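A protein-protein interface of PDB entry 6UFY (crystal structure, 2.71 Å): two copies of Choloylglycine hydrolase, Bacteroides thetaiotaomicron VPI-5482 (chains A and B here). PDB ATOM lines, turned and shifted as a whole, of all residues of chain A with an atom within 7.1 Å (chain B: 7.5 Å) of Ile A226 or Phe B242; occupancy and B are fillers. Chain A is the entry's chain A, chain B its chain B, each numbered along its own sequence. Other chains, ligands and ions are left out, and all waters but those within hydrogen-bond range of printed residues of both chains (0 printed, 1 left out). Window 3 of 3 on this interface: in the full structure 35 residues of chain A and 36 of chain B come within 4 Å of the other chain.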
ATOM      1  N   TYR A   7      21.571  11.212  -2.164  1.00  0.00           N
ATOM      2  CA  TYR A   7      20.266  11.829  -2.363  1.00  0.00           C
ATOM      3  C   TYR A   7      19.387  11.572  -1.146  1.00  0.00           C
ATOM      4  O   TYR A   7      19.301  10.438  -0.664  1.00  0.00           O
ATOM      5  CB  TYR A   7      19.597  11.283  -3.625  1.00  0.00           C
ATOM      6  CG  TYR A   7      18.112  11.554  -3.713  1.00  0.00           C
ATOM      7  CD1 TYR A   7      17.634  12.823  -4.015  1.00  0.00           C
ATOM      8  CD2 TYR A   7      17.188  10.538  -3.507  1.00  0.00           C
ATOM      9  CE1 TYR A   7      16.278  13.073  -4.101  1.00  0.00           C
ATOM     10  CE2 TYR A   7      15.829  10.779  -3.592  1.00  0.00           C
ATOM     11  CZ  TYR A   7      15.380  12.049  -3.890  1.00  0.00           C
ATOM     12  OH  TYR A   7      14.029  12.299  -3.976  1.00  0.00           O
ATOM     13  N   MET A  13      14.024   8.153   2.180  1.00  0.00           N
ATOM     14  CA  MET A  13      14.540   7.746   0.875  1.00  0.00           C
ATOM     15  C   MET A  13      15.985   8.218   0.777  1.00  0.00           C
ATOM     16  O   MET A  13      16.254   9.383   0.476  1.00  0.00           O
ATOM     17  CB  MET A  13      13.686   8.313  -0.254  1.00  0.00           C
ATOM     18  CG  MET A  13      13.975   7.689  -1.611  1.00  0.00           C
ATOM     19  SD  MET A  13      13.627   5.918  -1.637  1.00  0.00           S
ATOM     20  CE  MET A  13      14.159   5.479  -3.291  1.00  0.00           C
ATOM     21  N   TYR A 214      23.242  19.153  -8.881  1.00  0.00           N
ATOM     22  CA  TYR A 214      22.239  18.313  -9.529  1.00  0.00           C
ATOM     23  C   TYR A 214      21.544  17.377  -8.549  1.00  0.00           C
ATOM     24  O   TYR A 214      20.378  17.027  -8.757  1.00  0.00           O
ATOM     25  CB  TYR A 214      22.881  17.513 -10.663  1.00  0.00           C
ATOM     26  CG  TYR A 214      23.099  18.310 -11.927  1.00  0.00           C
ATOM     27  CD1 TYR A 214      22.224  19.323 -12.292  1.00  0.00           C
ATOM     28  CD2 TYR A 214      24.184  18.049 -12.755  1.00  0.00           C
ATOM     29  CE1 TYR A 214      22.421  20.053 -13.448  1.00  0.00           C
ATOM     30  CE2 TYR A 214      24.388  18.773 -13.912  1.00  0.00           C
ATOM     31  CZ  TYR A 214      23.504  19.774 -14.254  1.00  0.00           C
ATOM     32  OH  TYR A 214      23.707  20.499 -15.406  1.00  0.00           O
ATOM     33  N   ALA A 217      18.519  19.041  -7.222  1.00  0.00           N
ATOM     34  CA  ALA A 217      17.549  19.506  -8.203  1.00  0.00           C
ATOM     35  C   ALA A 217      16.710  18.389  -8.810  1.00  0.00           C
ATOM     36  O   ALA A 217      15.671  18.678  -9.413  1.00  0.00           O
ATOM     37  CB  ALA A 217      18.259  20.266  -9.330  1.00  0.00           C
ATOM     38  N   ILE A 218      17.129  17.133  -8.670  1.00  0.00           N
ATOM     39  CA  ILE A 218      16.361  15.992  -9.165  1.00  0.00           C
ATOM     40  C   ILE A 218      15.047  15.924  -8.391  1.00  0.00           C
ATOM     41  O   ILE A 218      14.949  16.511  -7.304  1.00  0.00           O
ATOM     42  CB  ILE A 218      17.164  14.686  -9.045  1.00  0.00           C
ATOM     43  CG1 ILE A 218      17.714  14.513  -7.629  1.00  0.00           C
ATOM     44  CG2 ILE A 218      18.286  14.654 -10.073  1.00  0.00           C
ATOM     45  CD1 ILE A 218      18.515  13.241  -7.442  1.00  0.00           C
ATOM     46  N   PRO A 219      14.016  15.245  -8.904  1.00  0.00           N
ATOM     47  CA  PRO A 219      12.719  15.248  -8.216  1.00  0.00           C
ATOM     48  C   PRO A 219      12.817  14.733  -6.788  1.00  0.00           C
ATOM     49  O   PRO A 219      13.649  13.885  -6.458  1.00  0.00           O
ATOM     50  CB  PRO A 219      11.856  14.323  -9.082  1.00  0.00           C
ATOM     51  CG  PRO A 219      12.465  14.405 -10.432  1.00  0.00           C
ATOM     52  CD  PRO A 219      13.942  14.551 -10.203  1.00  0.00           C
ATOM     53  N   THR A 221      11.198  12.585  -4.562  1.00  0.00           N
ATOM     54  CA  THR A 221      10.261  11.474  -4.595  1.00  0.00           C
ATOM     55  C   THR A 221      10.756  10.339  -3.710  1.00  0.00           C
ATOM     56  O   THR A 221      11.953  10.204  -3.442  1.00  0.00           O
ATOM     57  CB  THR A 221      10.054  10.955  -6.024  1.00  0.00           C
ATOM     58  OG1 THR A 221       9.241   9.776  -5.994  1.00  0.00           O
ATOM     59  CG2 THR A 221      11.394  10.628  -6.668  1.00  0.00           C
ATOM     60  N   ALA A 222       9.806   9.525  -3.257  1.00  0.00           N
ATOM     61  CA  ALA A 222      10.096   8.315  -2.502  1.00  0.00           C
ATOM     62  C   ALA A 222       9.936   7.054  -3.338  1.00  0.00           C
ATOM     63  O   ALA A 222      10.171   5.954  -2.831  1.00  0.00           O
ATOM     64  CB  ALA A 222       9.196   8.233  -1.265  1.00  0.00           C
ATOM     65  N   ASP A 223       9.539   7.190  -4.602  1.00  0.00           N
ATOM     66  CA  ASP A 223       9.391   6.046  -5.492  1.00  0.00           C
ATOM     67  C   ASP A 223      10.751   5.679  -6.072  1.00  0.00           C
ATOM     68  O   ASP A 223      11.425   6.524  -6.671  1.00  0.00           O
ATOM     69  CB  ASP A 223       8.394   6.369  -6.604  1.00  0.00           C
ATOM     70  CG  ASP A 223       8.222   5.227  -7.589  1.00  0.00           C
ATOM     71  OD1 ASP A 223       8.811   4.148  -7.365  1.00  0.00           O
ATOM     72  OD2 ASP A 223       7.497   5.411  -8.590  1.00  0.00           O
ATOM     73  N   ALA A 224      11.153   4.417  -5.897  1.00  0.00           N
ATOM     74  CA  ALA A 224      12.457   3.982  -6.390  1.00  0.00           C
ATOM     75  C   ALA A 224      12.517   3.984  -7.912  1.00  0.00           C
ATOM     76  O   ALA A 224      13.605   4.103  -8.486  1.00  0.00           O
ATOM     77  CB  ALA A 224      12.788   2.592  -5.849  1.00  0.00           C
ATOM     78  N   LYS A 225      11.367   3.862  -8.580  1.00  0.00           N
ATOM     79  CA  LYS A 225      11.346   3.869 -10.039  1.00  0.00           C
ATOM     80  C   LYS A 225      11.784   5.207 -10.620  1.00  0.00           C
ATOM     81  O   LYS A 225      12.099   5.278 -11.812  1.00  0.00           O
ATOM     82  CB  LYS A 225       9.946   3.518 -10.548  1.00  0.00           C
ATOM     83  CG  LYS A 225       9.580   2.046 -10.421  1.00  0.00           C
ATOM     84  CD  LYS A 225      10.525   1.174 -11.233  1.00  0.00           C
ATOM     85  CE  LYS A 225      10.050  -0.270 -11.279  1.00  0.00           C
ATOM     86  NZ  LYS A 225       8.764  -0.413 -12.016  1.00  0.00           N
ATOM     87  N   ILE A 226      11.810   6.263  -9.811  1.00  0.00           N
ATOM     88  CA  ILE A 226      12.227   7.582 -10.255  1.00  0.00           C
ATOM     89  C   ILE A 226      13.535   8.010  -9.599  1.00  0.00           C
ATOM     90  O   ILE A 226      14.404   8.583 -10.260  1.00  0.00           O
ATOM     91  CB  ILE A 226      11.120   8.625  -9.991  1.00  0.00           C
ATOM     92  CG1 ILE A 226       9.766   8.107 -10.482  1.00  0.00           C
ATOM     93  CG2 ILE A 226      11.471   9.954 -10.652  1.00  0.00           C
ATOM     94  CD1 ILE A 226       8.603   9.016 -10.143  1.00  0.00           C
ATOM     95  N   ALA A 227      13.690   7.738  -8.302  1.00  0.00           N
ATOM     96  CA  ALA A 227      14.867   8.211  -7.580  1.00  0.00           C
ATOM     97  C   ALA A 227      16.140   7.558  -8.105  1.00  0.00           C
ATOM     98  O   ALA A 227      17.129   8.242  -8.389  1.00  0.00           O
ATOM     99  CB  ALA A 227      14.703   7.951  -6.082  1.00  0.00           C
ATOM    100  N   VAL A 228      16.132   6.230  -8.247  1.00  0.00           N
ATOM    101  CA  VAL A 228      17.337   5.524  -8.690  1.00  0.00           C
ATOM    102  C   VAL A 228      17.781   5.955 -10.084  1.00  0.00           C
ATOM    103  O   VAL A 228      18.981   6.211 -10.272  1.00  0.00           O
ATOM    104  CB  VAL A 228      17.131   4.003  -8.574  1.00  0.00           C
ATOM    105  CG1 VAL A 228      18.369   3.262  -9.049  1.00  0.00           C
ATOM    106  CG2 VAL A 228      16.789   3.619  -7.141  1.00  0.00           C
ATOM    107  N   PRO A 229      16.903   6.050 -11.094  1.00  0.00           N
ATOM    108  CA  PRO A 229      17.381   6.516 -12.408  1.00  0.00           C
ATOM    109  C   PRO A 229      17.919   7.938 -12.393  1.00  0.00           C
ATOM    110  O   PRO A 229      18.924   8.218 -13.060  1.00  0.00           O
ATOM    111  CB  PRO A 229      16.136   6.388 -13.298  1.00  0.00           C
ATOM    112  CG  PRO A 229      15.289   5.373 -12.626  1.00  0.00           C
ATOM    113  CD  PRO A 229      15.502   5.591 -11.163  1.00  0.00           C
ATOM    114  N   SER A 230      17.281   8.848 -11.652  1.00  0.00           N
ATOM    115  CA  SER A 230      17.756  10.227 -11.599  1.00  0.00           C
ATOM    116  C   SER A 230      19.040  10.367 -10.787  1.00  0.00           C
ATOM    117  O   SER A 230      19.889  11.199 -11.126  1.00  0.00           O
ATOM    118  CB  SER A 230      16.668  11.141 -11.031  1.00  0.00           C
ATOM    119  OG  SER A 230      16.100  10.605  -9.850  1.00  0.00           O
ATOM    120  N   VAL A 231      19.201   9.581  -9.720  1.00  0.00           N
ATOM    121  CA  VAL A 231      20.478   9.561  -9.010  1.00  0.00           C
ATOM    122  C   VAL A 231      21.562   8.976  -9.904  1.00  0.00           C
ATOM    123  O   VAL A 231      22.705   9.450  -9.916  1.00  0.00           O
ATOM    124  CB  VAL A 231      20.353   8.782  -7.687  1.00  0.00           C
ATOM    125  CG1 VAL A 231      21.728   8.552  -7.066  1.00  0.00           C
ATOM    126  CG2 VAL A 231      19.457   9.529  -6.719  1.00  0.00           C
ATOM    127  N   LEU A 232      21.219   7.942 -10.673  1.00  0.00           N
ATOM    128  CA  LEU A 232      22.157   7.419 -11.656  1.00  0.00           C
ATOM    129  C   LEU A 232      22.455   8.458 -12.730  1.00  0.00           C
ATOM    130  O   LEU A 232      23.590   8.557 -13.208  1.00  0.00           O
ATOM    131  CB  LEU A 232      21.604   6.136 -12.280  1.00  0.00           C
ATOM    132  CG  LEU A 232      22.562   5.340 -13.169  1.00  0.00           C
ATOM    133  CD1 LEU A 232      23.693   4.734 -12.352  1.00  0.00           C
ATOM    134  CD2 LEU A 232      21.812   4.258 -13.927  1.00  0.00           C
ATOM    135  N   SER A 233      21.452   9.259 -13.104  1.00  0.00           N
ATOM    136  CA  SER A 233      21.646  10.253 -14.157  1.00  0.00           C
ATOM    137  C   SER A 233      22.696  11.283 -13.762  1.00  0.00           C
ATOM    138  O   SER A 233      23.549  11.653 -14.579  1.00  0.00           O
ATOM    139  CB  SER A 233      20.321  10.943 -14.483  1.00  0.00           C
ATOM    140  OG  SER A 233      19.927  11.810 -13.434  1.00  0.00           O
ATOM    141  N   VAL A 234      22.654  11.763 -12.516  1.00  0.00           N
ATOM    142  CA  VAL A 234      23.665  12.712 -12.068  1.00  0.00           C
ATOM    143  C   VAL A 234      25.016  12.035 -11.889  1.00  0.00           C
ATOM    144  O   VAL A 234      26.049  12.713 -11.897  1.00  0.00           O
ATOM    145  CB  VAL A 234      23.226  13.421 -10.770  1.00  0.00           C
ATOM    146  CG1 VAL A 234      21.812  13.964 -10.910  1.00  0.00           C
ATOM    147  CG2 VAL A 234      23.335  12.491  -9.576  1.00  0.00           C
ATOM    148  N   TRP B  22      13.300  16.391 -23.337  1.00  0.00           N
ATOM    149  CA  TRP B  22      11.942  16.907 -23.389  1.00  0.00           C
ATOM    150  C   TRP B  22      11.433  17.118 -21.972  1.00  0.00           C
ATOM    151  O   TRP B  22      11.843  16.421 -21.039  1.00  0.00           O
ATOM    152  CB  TRP B  22      11.013  15.961 -24.163  1.00  0.00           C
ATOM    153  CG  TRP B  22       9.714  16.592 -24.564  1.00  0.00           C
ATOM    154  CD1 TRP B  22       8.507  16.447 -23.946  1.00  0.00           C
ATOM    155  CD2 TRP B  22       9.493  17.477 -25.671  1.00  0.00           C
ATOM    156  NE1 TRP B  22       7.548  17.182 -24.600  1.00  0.00           N
ATOM    157  CE2 TRP B  22       8.128  17.824 -25.662  1.00  0.00           C
ATOM    158  CE3 TRP B  22      10.317  18.008 -26.670  1.00  0.00           C
ATOM    159  CZ2 TRP B  22       7.567  18.677 -26.611  1.00  0.00           C
ATOM    160  CZ3 TRP B  22       9.758  18.854 -27.612  1.00  0.00           C
ATOM    161  CH2 TRP B  22       8.395  19.180 -27.575  1.00  0.00           C
ATOM    162  N   LYS B  23      10.526  18.087 -21.820  1.00  0.00           N
ATOM    163  CA  LYS B  23      10.019  18.433 -20.496  1.00  0.00           C
ATOM    164  C   LYS B  23       9.069  17.376 -19.944  1.00  0.00           C
ATOM    165  O   LYS B  23       9.005  17.184 -18.725  1.00  0.00           O
ATOM    166  CB  LYS B  23       9.327  19.795 -20.540  1.00  0.00           C
ATOM    167  CG  LYS B  23      10.283  20.964 -20.692  1.00  0.00           C
ATOM    168  CD  LYS B  23       9.530  22.275 -20.820  1.00  0.00           C
ATOM    169  CE  LYS B  23      10.486  23.450 -20.767  1.00  0.00           C
ATOM    170  NZ  LYS B  23      11.584  23.306 -21.761  1.00  0.00           N
ATOM    171  N   GLU B  24       8.318  16.689 -20.804  1.00  0.00           N
ATOM    172  CA  GLU B  24       7.438  15.621 -20.342  1.00  0.00           C
ATOM    173  C   GLU B  24       7.752  14.309 -21.049  1.00  0.00           C
ATOM    174  O   GLU B  24       8.774  14.192 -21.733  1.00  0.00           O
ATOM    175  CB  GLU B  24       5.969  15.991 -20.575  1.00  0.00           C
ATOM    176  CG  GLU B  24       5.591  16.076 -22.041  1.00  0.00           C
ATOM    177  CD  GLU B  24       4.098  16.015 -22.263  1.00  0.00           C
ATOM    178  OE1 GLU B  24       3.349  16.442 -21.363  1.00  0.00           O
ATOM    179  OE2 GLU B  24       3.676  15.532 -23.334  1.00  0.00           O
ATOM    180  N   ASP B  25       6.886  13.311 -20.879  1.00  0.00           N
ATOM    181  CA  ASP B  25       7.065  12.028 -21.549  1.00  0.00           C
ATOM    182  C   ASP B  25       6.846  12.212 -23.046  1.00  0.00           C
ATOM    183  O   ASP B  25       5.730  12.500 -23.489  1.00  0.00           O
ATOM    184  CB  ASP B  25       6.106  10.992 -20.971  1.00  0.00           C
ATOM    185  CG  ASP B  25       6.416   9.576 -21.439  1.00  0.00           C
ATOM    186  OD1 ASP B  25       7.329   9.395 -22.272  1.00  0.00           O
ATOM    187  OD2 ASP B  25       5.743   8.636 -20.965  1.00  0.00           O
ATOM    188  N   SER B 239      24.088  14.843 -21.515  1.00  0.00           N
ATOM    189  CA  SER B 239      22.695  14.666 -21.152  1.00  0.00           C
ATOM    190  C   SER B 239      22.309  15.591 -19.999  1.00  0.00           C
ATOM    191  O   SER B 239      23.157  16.107 -19.267  1.00  0.00           O
ATOM    192  CB  SER B 239      22.406  13.216 -20.752  1.00  0.00           C
ATOM    193  OG  SER B 239      22.403  12.339 -21.867  1.00  0.00           O
ATOM    194  N   VAL B 240      21.008  15.781 -19.832  1.00  0.00           N
ATOM    195  CA  VAL B 240      20.455  16.585 -18.743  1.00  0.00           C
ATOM    196  C   VAL B 240      19.904  15.634 -17.686  1.00  0.00           C
ATOM    197  O   VAL B 240      19.126  14.730 -18.031  1.00  0.00           O
ATOM    198  CB  VAL B 240      19.361  17.548 -19.248  1.00  0.00           C
ATOM    199  CG1 VAL B 240      18.808  18.400 -18.094  1.00  0.00           C
ATOM    200  CG2 VAL B 240      19.911  18.441 -20.343  1.00  0.00           C
ATOM    201  N   PRO B 241      20.282  15.786 -16.412  1.00  0.00           N
ATOM    202  CA  PRO B 241      19.770  14.873 -15.383  1.00  0.00           C
ATOM    203  C   PRO B 241      18.249  14.881 -15.349  1.00  0.00           C
ATOM    204  O   PRO B 241      17.601  15.861 -15.720  1.00  0.00           O
ATOM    205  CB  PRO B 241      20.370  15.424 -14.084  1.00  0.00           C
ATOM    206  CG  PRO B 241      21.605  16.139 -14.519  1.00  0.00           C
ATOM    207  CD  PRO B 241      21.279  16.728 -15.869  1.00  0.00           C
ATOM    208  N   PHE B 242      17.680  13.761 -14.913  1.00  0.00           N
ATOM    209  CA  PHE B 242      16.242  13.559 -15.031  1.00  0.00           C
ATOM    210  C   PHE B 242      15.485  14.424 -14.030  1.00  0.00           C
ATOM    211  O   PHE B 242      15.820  14.461 -12.843  1.00  0.00           O
ATOM    212  CB  PHE B 242      15.898  12.087 -14.820  1.00  0.00           C
ATOM    213  CG  PHE B 242      14.454  11.766 -15.058  1.00  0.00           C
ATOM    214  CD1 PHE B 242      13.970  11.618 -16.347  1.00  0.00           C
ATOM    215  CD2 PHE B 242      13.579  11.612 -13.996  1.00  0.00           C
ATOM    216  CE1 PHE B 242      12.641  11.325 -16.573  1.00  0.00           C
ATOM    217  CE2 PHE B 242      12.248  11.318 -14.216  1.00  0.00           C
ATOM    218  CZ  PHE B 242      11.778  11.175 -15.507  1.00  0.00           C
ATOM    219  N   GLY B 243      14.460  15.118 -14.517  1.00  0.00           N
ATOM    220  CA  GLY B 243      13.579  15.893 -13.661  1.00  0.00           C
ATOM    221  C   GLY B 243      14.220  17.086 -12.986  1.00  0.00           C
ATOM    222  O   GLY B 243      13.877  17.401 -11.838  1.00  0.00           O
ATOM    223  N   ILE B 244      15.140  17.765 -13.671  1.00  0.00           N
ATOM    224  CA  ILE B 244      15.816  18.916 -13.083  1.00  0.00           C
ATOM    225  C   ILE B 244      14.836  20.074 -12.958  1.00  0.00           C
ATOM    226  O   ILE B 244      14.191  20.473 -13.937  1.00  0.00           O
ATOM    227  CB  ILE B 244      17.037  19.313 -13.924  1.00  0.00           C
ATOM    228  CG1 ILE B 244      18.153  18.284 -13.760  1.00  0.00           C
ATOM    229  CG2 ILE B 244      17.533  20.694 -13.531  1.00  0.00           C
ATOM    230  CD1 ILE B 244      18.610  18.109 -12.329  1.00  0.00           C
ATOM    231  N   ASN B 245      14.721  20.620 -11.748  1.00  0.00           N
ATOM    232  CA  ASN B 245      13.889  21.792 -11.517  1.00  0.00           C
ATOM    233  C   ASN B 245      14.467  22.594 -10.362  1.00  0.00           C
ATOM    234  O   ASN B 245      15.148  22.054  -9.485  1.00  0.00           O
ATOM    235  CB  ASN B 245      12.429  21.414 -11.222  1.00  0.00           C
ATOM    236  CG  ASN B 245      12.232  20.864  -9.819  1.00  0.00           C
ATOM    237  OD1 ASN B 245      12.137  21.620  -8.849  1.00  0.00           O
ATOM    238  ND2 ASN B 245      12.150  19.544  -9.708  1.00  0.00           N
ATOM    239  N   ILE B 252      12.243  22.049 -16.861  1.00  0.00           N
ATOM    240  CA  ILE B 252      13.479  22.079 -17.633  1.00  0.00           C
ATOM    241  C   ILE B 252      13.540  20.822 -18.492  1.00  0.00           C
ATOM    242  O   ILE B 252      13.115  19.744 -18.061  1.00  0.00           O
ATOM    243  CB  ILE B 252      14.711  22.184 -16.707  1.00  0.00           C
ATOM    244  CG1 ILE B 252      14.626  23.454 -15.855  1.00  0.00           C
ATOM    245  CG2 ILE B 252      15.998  22.182 -17.508  1.00  0.00           C
ATOM    246  CD1 ILE B 252      15.638  23.517 -14.736  1.00  0.00           C
ATOM    247  N   SER B 253      14.058  20.964 -19.711  1.00  0.00           N
ATOM    248  CA  SER B 253      14.097  19.867 -20.675  1.00  0.00           C
ATOM    249  C   SER B 253      15.041  18.775 -20.180  1.00  0.00           C
ATOM    250  O   SER B 253      16.261  18.956 -20.169  1.00  0.00           O
ATOM    251  CB  SER B 253      14.533  20.394 -22.038  1.00  0.00           C
ATOM    252  OG  SER B 253      14.258  19.458 -23.064  1.00  0.00           O
ATOM    253  N   SER B 254      14.479  17.637 -19.777  1.00  0.00           N
ATOM    254  CA  SER B 254      15.247  16.517 -19.253  1.00  0.00           C
ATOM    255  C   SER B 254      15.471  15.459 -20.327  1.00  0.00           C
ATOM    256  O   SER B 254      14.633  15.256 -21.208  1.00  0.00           O
ATOM    257  CB  SER B 254      14.544  15.883 -18.049  1.00  0.00           C
ATOM    258  OG  SER B 254      14.883  16.549 -16.846  1.00  0.00           O
ATOM    259  N   THR B 255      16.612  14.780 -20.235  1.00  0.00           N
ATOM    260  CA  THR B 255      16.929  13.705 -21.167  1.00  0.00           C
ATOM    261  C   THR B 255      16.007  12.517 -20.930  1.00  0.00           C
ATOM    262  O   THR B 255      15.896  12.018 -19.806  1.00  0.00           O
ATOM    263  CB  THR B 255      18.389  13.278 -21.015  1.00  0.00           C
ATOM    264  OG1 THR B 255      19.245  14.404 -21.240  1.00  0.00           O
ATOM    265  CG2 THR B 255      18.732  12.182 -22.015  1.00  0.00           C
ATOM    266  N   ARG B 256      15.341  12.065 -21.989  1.00  0.00           N
ATOM    267  CA  ARG B 256      14.397  10.957 -21.897  1.00  0.00           C
ATOM    268  C   ARG B 256      14.933   9.659 -22.478  1.00  0.00           C
ATOM    269  O   ARG B 256      14.741   8.599 -21.878  1.00  0.00           O
ATOM    270  CB  ARG B 256      13.078  11.325 -22.591  1.00  0.00           C
ATOM    271  CG  ARG B 256      12.501  12.665 -22.146  1.00  0.00           C
ATOM    272  CD  ARG B 256      12.563  12.827 -20.632  1.00  0.00           C
ATOM    273  NE  ARG B 256      11.406  12.254 -19.954  1.00  0.00           N
ATOM    274  CZ  ARG B 256      10.555  12.958 -19.216  1.00  0.00           C
ATOM    275  NH1 ARG B 256      10.737  14.261 -19.049  1.00  0.00           N
ATOM    276  NH2 ARG B 256       9.526  12.356 -18.633  1.00  0.00           N
ATOM    277  N   THR B 273      16.207   6.766 -20.130  1.00  0.00           N
ATOM    278  CA  THR B 273      16.711   7.242 -18.847  1.00  0.00           C
ATOM    279  C   THR B 273      16.128   6.442 -17.689  1.00  0.00           C
ATOM    280  O   THR B 273      16.842   6.094 -16.741  1.00  0.00           O
ATOM    281  CB  THR B 273      16.402   8.732 -18.684  1.00  0.00           C
ATOM    282  OG1 THR B 273      17.141   9.483 -19.655  1.00  0.00           O
ATOM    283  CG2 THR B 273      16.771   9.212 -17.289  1.00  0.00           C
ATOM    284  N   LEU B 274      14.836   6.128 -17.752  1.00  0.00           N
ATOM    285  CA  LEU B 274      14.172   5.410 -16.672  1.00  0.00           C
ATOM    286  C   LEU B 274      14.187   3.898 -16.862  1.00  0.00           C
ATOM    287  O   LEU B 274      13.727   3.175 -15.971  1.00  0.00           O
ATOM    288  CB  LEU B 274      12.728   5.902 -16.517  1.00  0.00           C
ATOM    289  CG  LEU B 274      12.530   7.402 -16.270  1.00  0.00           C
ATOM    290  CD1 LEU B 274      11.140   7.671 -15.709  1.00  0.00           C
ATOM    291  CD2 LEU B 274      13.601   7.973 -15.350  1.00  0.00           C
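The backbone carbonyl oxygen of Gly B243 sits close to the backbone carbonyl oxygen of Ala A217 (3.3 Å). O of Ala A217 lies within hydrogen-bond range of N of Asn B245. The backbone NH of Phe B242 lies within hydrogen-bond range of the side-chain hydroxyl of Ser A233.
OG of Ser B254 lies within hydrogen-bond range of O of Pro B241, 3.0 Å away. The side-chain hydroxyl of Tyr A7 is in hydrogen-bond range of the backbone carbonyl oxygen of Pro A219 (3.0 Å). OG1 of Thr B273 sits at hydrogen-bond distance from O of Thr B255 (2.8 Å). O of Gly B243 is in hydrogen-bond range of ND2 of Asn B245 (3.5 Å). O of Ile A226 sits at hydrogen-bond distance from OG of Ser A230 (2.7 Å). The backbone NH (N) of Ile B244 sits at hydrogen-bond distance from the side-chain hydroxyl (OG) of Ser B254, 3.4 Å away.
Among the printed residues, merely in contact across the chains: Pro A219 with Phe B242 (3.2 Å), Pro A219 with Gly B243 (3.3 Å), Pro A229 with Thr B273 (3.5 Å), Pro A229 with Leu B274 (3.6 Å), Ser A233 with Pro B241 (3.6 Å), Tyr A214 with Pro B241 (3.7 Å), Ala A217 with Ile B244 (3.7 Å), Ile A218 with Phe B242 (3.7 Å), Val A234 with Pro B241 (3.8 Å), Tyr A214 with Ile B244 (3.8 Å), Ser A230 with Phe B242 (3.9 Å), Ile A226 with Phe B242 (3.9 Å) and Ile A218 with Gly B243 (3.9 Å).
Printed residues of chain B within 4 Å of Ile A226: Phe B242. Of the printed residues of chain B, Val A234 touches Pro B241 (3.8 Å). Glu B24 touches none of the printed residues of chain A. Of the printed residues of chain A, Phe B242 touches Ile A218, Pro A219, Ile A226, Ser A230 and Ser A233. Of the printed residues of chain A, Asn B245 touches Ala A217. Ser B254 touches none of the printed residues of chain A. Printed residues of chain A within 4 Å of Thr B273: Pro A229. The nearest printed residue of chain B that does not touch Ala A217 is Phe B242 (5.4 Å).
Of the 20 printed residues of chain A, 9 touch a printed residue of chain B. Hydrophobic or aromatic side chains of chain A that line the printed part of chain B: Tyr A214, Ala A217, Ile A218, Pro A219, Ile A226, Pro A229 and Val A234. Of the 18 printed residues of chain B, 7 touch a printed residue of chain A. Printed residues of chain B that touch a printed residue of chain A: Pro B241, Phe B242, Gly B243, Ile B244, Asn B245, Thr B273 and Leu B274. Hydrophobic or aromatic side chains of chain B that line the printed part of chain A: Pro B241, Phe B242, Ile B244 and Leu B274. Along chain B the printed residues that touch a printed residue of chain A span positions 241 to 274. Among the printed residues, 16 pairs touch across the chains. Among the printed residues, no Asp or Glu carboxylate lies within 4 Å of a Lys or Arg side-chain nitrogen of the other chain.
No position is printed for both chains.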
